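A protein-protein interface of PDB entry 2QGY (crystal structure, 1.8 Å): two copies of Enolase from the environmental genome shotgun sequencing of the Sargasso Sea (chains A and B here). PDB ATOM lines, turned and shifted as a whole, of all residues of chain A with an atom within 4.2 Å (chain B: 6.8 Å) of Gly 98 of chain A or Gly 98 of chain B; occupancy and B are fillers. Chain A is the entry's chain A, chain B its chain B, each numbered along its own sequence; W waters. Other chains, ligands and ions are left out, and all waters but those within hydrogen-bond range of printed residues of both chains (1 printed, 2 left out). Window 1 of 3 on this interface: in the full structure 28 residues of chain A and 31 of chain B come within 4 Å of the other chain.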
ATOM      1  N   ARG A  97      19.488   3.302   3.523  1.00  0.00           N
ATOM      2  CA  ARG A  97      18.461   2.563   4.267  1.00  0.00           C
ATOM      3  C   ARG A  97      19.029   1.914   5.524  1.00  0.00           C
ATOM      4  O   ARG A  97      19.728   2.572   6.304  1.00  0.00           O
ATOM      5  CB  ARG A  97      17.755   1.551   3.359  1.00  0.00           C
ATOM      6  CG  ARG A  97      16.952   2.178   2.234  1.00  0.00           C
ATOM      7  CD  ARG A  97      16.196   1.111   1.407  1.00  0.00           C
ATOM      8  NE  ARG A  97      17.104   0.283   0.613  1.00  0.00           N
ATOM      9  CZ  ARG A  97      17.448   0.530  -0.659  1.00  0.00           C
ATOM     10  NH1 ARG A  97      18.297  -0.277  -1.284  1.00  0.00           N
ATOM     11  NH2 ARG A  97      16.948   1.573  -1.318  1.00  0.00           N
ATOM     12  N   GLY A  98      18.725   0.641   5.732  1.00  0.00           N
ATOM     13  CA  GLY A  98      19.328  -0.126   6.823  1.00  0.00           C
ATOM     14  C   GLY A  98      18.274  -0.357   7.872  1.00  0.00           C
ATOM     15  O   GLY A  98      17.309   0.408   7.957  1.00  0.00           O
ATOM     16  N   LEU A  99      18.459  -1.391   8.685  1.00  0.00           N
ATOM     17  CA  LEU A  99      17.424  -1.828   9.624  1.00  0.00           C
ATOM     18  C   LEU A  99      17.105  -0.793  10.682  1.00  0.00           C
ATOM     19  O   LEU A  99      15.932  -0.576  10.982  1.00  0.00           O
ATOM     20  CB  LEU A  99      17.826  -3.138  10.300  1.00  0.00           C
ATOM     21  CG  LEU A  99      17.666  -4.425   9.507  1.00  0.00           C
ATOM     22  CD1 LEU A  99      17.718  -5.595  10.485  1.00  0.00           C
ATOM     23  CD2 LEU A  99      16.317  -4.467   8.698  1.00  0.00           C
ATOM     24  N   ASP A 100      18.145  -0.164  11.256  1.00  0.00           N
ATOM     25  CA  ASP A 100      17.965   0.835  12.302  1.00  0.00           C
ATOM     26  C   ASP A 100      17.083   1.984  11.793  1.00  0.00           C
ATOM     27  O   ASP A 100      16.108   2.364  12.451  1.00  0.00           O
ATOM     28  CB  ASP A 100      19.327   1.348  12.801  1.00  0.00           C
ATOM     29  CG  ASP A 100      20.259   0.205  13.196  1.00  0.00           C
ATOM     30  OD1 ASP A 100      20.420   0.001  14.423  1.00  0.00           O
ATOM     31  OD2 ASP A 100      20.811  -0.513  12.292  1.00  0.00           O
ATOM     32  N   PHE A 101      17.380   2.507  10.599  1.00  0.00           N
ATOM     33  CA  PHE A 101      16.601   3.627  10.093  1.00  0.00           C
ATOM     34  C   PHE A 101      15.160   3.181   9.794  1.00  0.00           C
ATOM     35  O   PHE A 101      14.199   3.891  10.120  1.00  0.00           O
ATOM     36  CB  PHE A 101      17.270   4.218   8.845  1.00  0.00           C
ATOM     37  CG  PHE A 101      16.524   5.359   8.242  1.00  0.00           C
ATOM     38  CD1 PHE A 101      16.553   6.638   8.846  1.00  0.00           C
ATOM     39  CD2 PHE A 101      15.819   5.193   7.065  1.00  0.00           C
ATOM     40  CE1 PHE A 101      15.860   7.702   8.277  1.00  0.00           C
ATOM     41  CE2 PHE A 101      15.143   6.267   6.499  1.00  0.00           C
ATOM     42  CZ  PHE A 101      15.172   7.517   7.110  1.00  0.00           C
ATOM     43  N   SER A 102      15.030   2.019   9.167  1.00  0.00           N
ATOM     44  CA  SER A 102      13.738   1.454   8.782  1.00  0.00           C
ATOM     45  C   SER A 102      12.909   1.161  10.031  1.00  0.00           C
ATOM     46  O   SER A 102      11.671   1.286   9.985  1.00  0.00           O
ATOM     47  CB  SER A 102      13.929   0.154   7.938  1.00  0.00           C
ATOM     48  OG  SER A 102      14.529   0.452   6.675  1.00  0.00           O
ATOM     49  N   SER A 255      15.039  -4.877   4.696  1.00  0.00           N
ATOM     50  CA  SER A 255      13.984  -3.869   4.618  1.00  0.00           C
ATOM     51  C   SER A 255      14.057  -3.189   3.275  1.00  0.00           C
ATOM     52  O   SER A 255      15.053  -3.322   2.550  1.00  0.00           O
ATOM     53  CB  SER A 255      14.077  -2.818   5.765  1.00  0.00           C
ATOM     54  OG  SER A 255      15.349  -2.160   5.751  1.00  0.00           O
ATOM     55  N   ARG B  59      20.678  11.355  11.090  1.00  0.00           N
ATOM     56  CA  ARG B  59      21.083  10.162  11.804  1.00  0.00           C
ATOM     57  C   ARG B  59      22.456  10.312  12.468  1.00  0.00           C
ATOM     58  O   ARG B  59      22.957   9.363  13.091  1.00  0.00           O
ATOM     59  CB  ARG B  59      21.070   9.006  10.799  1.00  0.00           C
ATOM     60  CG  ARG B  59      19.658   8.750  10.288  1.00  0.00           C
ATOM     61  CD  ARG B  59      19.655   8.542   8.768  1.00  0.00           C
ATOM     62  NE  ARG B  59      20.022   7.181   8.410  1.00  0.00           N
ATOM     63  CZ  ARG B  59      19.697   6.599   7.249  1.00  0.00           C
ATOM     64  NH1 ARG B  59      19.036   7.260   6.303  1.00  0.00           N
ATOM     65  NH2 ARG B  59      20.047   5.340   7.040  1.00  0.00           N
ATOM     66  N   HIS B  96      21.946  -8.414  11.699  1.00  0.00           N
ATOM     67  CA  HIS B  96      21.132  -7.193  11.541  1.00  0.00           C
ATOM     68  C   HIS B  96      22.054  -6.118  11.066  1.00  0.00           C
ATOM     69  O   HIS B  96      22.916  -5.644  11.825  1.00  0.00           O
ATOM     70  CB  HIS B  96      20.529  -6.766  12.863  1.00  0.00           C
ATOM     71  CG  HIS B  96      19.542  -7.750  13.410  1.00  0.00           C
ATOM     72  ND1 HIS B  96      19.813  -8.543  14.506  1.00  0.00           N
ATOM     73  CD2 HIS B  96      18.302  -8.095  12.990  1.00  0.00           C
ATOM     74  CE1 HIS B  96      18.765  -9.318  14.755  1.00  0.00           C
ATOM     75  NE2 HIS B  96      17.841  -9.073  13.841  1.00  0.00           N
ATOM     76  N   ARG B  97      21.868  -5.721   9.826  1.00  0.00           N
ATOM     77  CA  ARG B  97      22.820  -4.856   9.154  1.00  0.00           C
ATOM     78  C   ARG B  97      22.131  -3.578   8.720  1.00  0.00           C
ATOM     79  O   ARG B  97      20.910  -3.551   8.468  1.00  0.00           O
ATOM     80  CB  ARG B  97      23.372  -5.553   7.912  1.00  0.00           C
ATOM     81  CG  ARG B  97      24.134  -6.823   8.256  1.00  0.00           C
ATOM     82  CD  ARG B  97      24.873  -7.378   7.060  1.00  0.00           C
ATOM     83  NE  ARG B  97      23.980  -8.071   6.144  1.00  0.00           N
ATOM     84  CZ  ARG B  97      23.833  -9.396   6.069  1.00  0.00           C
ATOM     85  NH1 ARG B  97      24.517 -10.222   6.864  1.00  0.00           N
ATOM     86  NH2 ARG B  97      22.987  -9.889   5.186  1.00  0.00           N
ATOM     87  N   GLY B  98      22.900  -2.516   8.600  1.00  0.00           N
ATOM     88  CA  GLY B  98      22.367  -1.292   7.977  1.00  0.00           C
ATOM     89  C   GLY B  98      23.461  -0.248   7.934  1.00  0.00           C
ATOM     90  O   GLY B  98      24.476  -0.418   8.595  1.00  0.00           O
ATOM     91  N   LEU B  99      23.264   0.816   7.152  1.00  0.00           N
ATOM     92  CA  LEU B  99      24.340   1.808   6.978  1.00  0.00           C
ATOM     93  C   LEU B  99      24.691   2.554   8.238  1.00  0.00           C
ATOM     94  O   LEU B  99      25.877   2.840   8.460  1.00  0.00           O
ATOM     95  CB  LEU B  99      24.000   2.849   5.906  1.00  0.00           C
ATOM     96  CG  LEU B  99      24.031   2.467   4.448  1.00  0.00           C
ATOM     97  CD1 LEU B  99      23.998   3.788   3.631  1.00  0.00           C
ATOM     98  CD2 LEU B  99      25.302   1.645   4.098  1.00  0.00           C
ATOM     99  N   ASP B 100      23.691   2.885   9.051  1.00  0.00           N
ATOM    100  CA  ASP B 100      23.978   3.595  10.291  1.00  0.00           C
ATOM    101  C   ASP B 100      24.899   2.785  11.217  1.00  0.00           C
ATOM    102  O   ASP B 100      25.878   3.314  11.765  1.00  0.00           O
ATOM    103  CB  ASP B 100      22.690   4.019  10.990  1.00  0.00           C
ATOM    104  CG  ASP B 100      21.764   4.776  10.059  1.00  0.00           C
ATOM    105  OD1 ASP B 100      21.771   6.019  10.149  1.00  0.00           O
ATOM    106  OD2 ASP B 100      21.048   4.139   9.236  1.00  0.00           O
ATOM    107  N   PHE B 101      24.577   1.504  11.373  1.00  0.00           N
ATOM    108  CA  PHE B 101      25.371   0.636  12.220  1.00  0.00           C
ATOM    109  C   PHE B 101      26.767   0.422  11.629  1.00  0.00           C
ATOM    110  O   PHE B 101      27.763   0.452  12.366  1.00  0.00           O
ATOM    111  CB  PHE B 101      24.700  -0.722  12.374  1.00  0.00           C
ATOM    112  CG  PHE B 101      25.419  -1.623  13.330  1.00  0.00           C
ATOM    113  CD1 PHE B 101      25.407  -1.332  14.693  1.00  0.00           C
ATOM    114  CD2 PHE B 101      26.092  -2.762  12.867  1.00  0.00           C
ATOM    115  CE1 PHE B 101      26.082  -2.128  15.594  1.00  0.00           C
ATOM    116  CE2 PHE B 101      26.789  -3.587  13.766  1.00  0.00           C
ATOM    117  CZ  PHE B 101      26.784  -3.277  15.116  1.00  0.00           C
ATOM    118  N   SER B 102      26.826   0.203  10.307  1.00  0.00           N
ATOM    119  CA  SER B 102      28.111  -0.004   9.619  1.00  0.00           C
ATOM    120  C   SER B 102      28.985   1.241   9.716  1.00  0.00           C
ATOM    121  O   SER B 102      30.198   1.126   9.883  1.00  0.00           O
ATOM    122  CB  SER B 102      27.894  -0.398   8.160  1.00  0.00           C
ATOM    123  OG  SER B 102      27.335  -1.724   8.140  1.00  0.00           O
ATOM    124  N   SER B 103      28.369   2.424   9.684  1.00  0.00           N
ATOM    125  CA  SER B 103      29.163   3.666   9.865  1.00  0.00           C
ATOM    126  C   SER B 103      29.758   3.726  11.274  1.00  0.00           C
ATOM    127  O   SER B 103      30.913   4.124  11.446  1.00  0.00           O
ATOM    128  CB  SER B 103      28.317   4.946   9.622  1.00  0.00           C
ATOM    129  OG  SER B 103      27.805   4.942   8.295  1.00  0.00           O
ATOM    130  N   LYS B 253      25.923   2.979  -1.134  1.00  0.00           N
ATOM    131  CA  LYS B 253      24.779   2.988  -0.209  1.00  0.00           C
ATOM    132  C   LYS B 253      24.527   1.656   0.486  1.00  0.00           C
ATOM    133  O   LYS B 253      23.512   1.500   1.170  1.00  0.00           O
ATOM    134  CB  LYS B 253      23.504   3.491  -0.915  1.00  0.00           C
ATOM    135  CG  LYS B 253      23.632   4.966  -1.263  1.00  0.00           C
ATOM    136  CD  LYS B 253      22.496   5.535  -1.970  1.00  0.00           C
ATOM    137  CE  LYS B 253      22.868   6.934  -2.509  1.00  0.00           C
ATOM    138  NZ  LYS B 253      22.275   7.008  -3.875  1.00  0.00           N
ATOM    139  N   SER B 255      26.356  -1.989   2.584  1.00  0.00           N
ATOM    140  CA  SER B 255      27.466  -2.427   3.407  1.00  0.00           C
ATOM    141  C   SER B 255      27.361  -3.927   3.634  1.00  0.00           C
ATOM    142  O   SER B 255      26.308  -4.538   3.356  1.00  0.00           O
ATOM    143  CB  SER B 255      27.445  -1.675   4.761  1.00  0.00           C
ATOM    144  OG  SER B 255      26.334  -2.085   5.565  1.00  0.00           O
ATOM    145  N   GLY B 278      31.877   3.675   5.740  1.00  0.00           N
ATOM    146  CA  GLY B 278      30.506   3.169   5.703  1.00  0.00           C
ATOM    147  C   GLY B 278      30.355   1.672   5.533  1.00  0.00           C
ATOM    148  O   GLY B 278      29.286   1.124   5.818  1.00  0.00           O
HETATM  149  O   HOH W   1      21.254   1.580   2.325  1.00  0.00           O
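Gly 98 of chain A touches one residue of chain B.
Of chain A, only Gly 98 and Leu 99 come within 4 Å of Gly 98 of chain B.
Of the printed residues of chain B, Phe 101 of chain A touches Arg 59 (3.5 Å) and Asp 100 (3.8 Å).
Of the printed residues of chain B, Arg 97 of chain A touches Arg 59 and Asp 100.
Of the printed residues of chain B, Asp 100 of chain A touches Phe 101 (3.9 Å).
Of the printed residues of chain A, Asp 100 of chain B touches Arg 97 and Phe 101.
Leu 99 of chain B touches none of the printed residues of chain A.
The nearest residue of chain B that does not touch Gly 98 of chain A is Leu 99 of chain B (4.1 Å).
The backbone carbonyl oxygen (O) of Arg 97 of chain A sits at hydrogen-bond distance from the guanidinium group (NH2) of Arg 59 of chain B (2.9 Å).
The backbone NH (N) of Leu 99 of chain A lies within hydrogen-bond range of the backbone carbonyl oxygen (O) of Arg 97 of chain B, 3.3 Å away.
Asp 100 of chain B touches Arg 97 of chain A.
CA of Gly 98 of chain A touches CA of Gly 98 of chain B (3.5 Å).
CD2 of His 96 of chain B touches CD1 of Leu 99 of chain A, 3.6 Å away.
N of Leu 99 of chain A touches CA of Gly 98 of chain B, at 3.97 Å.
Asp 100 of chain A touches Phe 101 of chain B (OD2 to CB, 3.9 Å).
CB of Phe 101 of chain A touches NH2 of Arg 59 of chain B, 3.5 Å away.
Phe 101 of chain A touches Asp 100 of chain B (CB to OD2, 3.8 Å).
The backbone carbonyl oxygen of Gly 98 of chain A sits at hydrogen-bond distance from the side-chain hydroxyl of Ser 102 of chain A (3.1 Å).
The guanidinium group of Arg 59 of chain B is in salt-bridge range of the side-chain carboxylate of Asp 100 of chain B (2.7 Å).
OG of Ser 102 of chain B lies within hydrogen-bond range of O of Gly 98 of chain B (3.2 Å).
Water W1 bridges O of Lys 253 of chain B and N of Arg 97 of chain A.
Gly 98 of chain A touches its own counterpart, Gly 98 of chain B.
Leu 99 of chain A touches Arg 97 of chain B, but with the chains exchanged Arg 97 of chain A does not touch Leu 99 of chain B (4.04 Å).
Leu 99 of chain A touches Gly 98 of chain B, but with the chains exchanged Gly 98 of chain A does not touch Leu 99 of chain B (4.1 Å).
Asp 100 of chain A touches Phe 101 of chain B, and with the chains exchanged Phe 101 of chain A touches Asp 100 of chain B.
Positions printed for both chains: 97, 98, 99, 100, 101, 102 and 255.
Of the 9 pairs that touch across the chains among the printed residues, 3 have their exchanged pair printed and touching as well.
Of the 12 printed residues of chain B, 6 touch a printed residue of chain A.
Hydrophobic or aromatic side chains of chain B within 4 Å of the printed part of chain A: His 96 and Phe 101.
Of the 7 printed residues of chain A, 5 touch a printed residue of chain B.
Hydrophobic or aromatic side chains of chain A within 4 Å of the printed part of chain B: Leu 99 and Phe 101.
Among the printed residues, 9 pairs touch across the chains.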
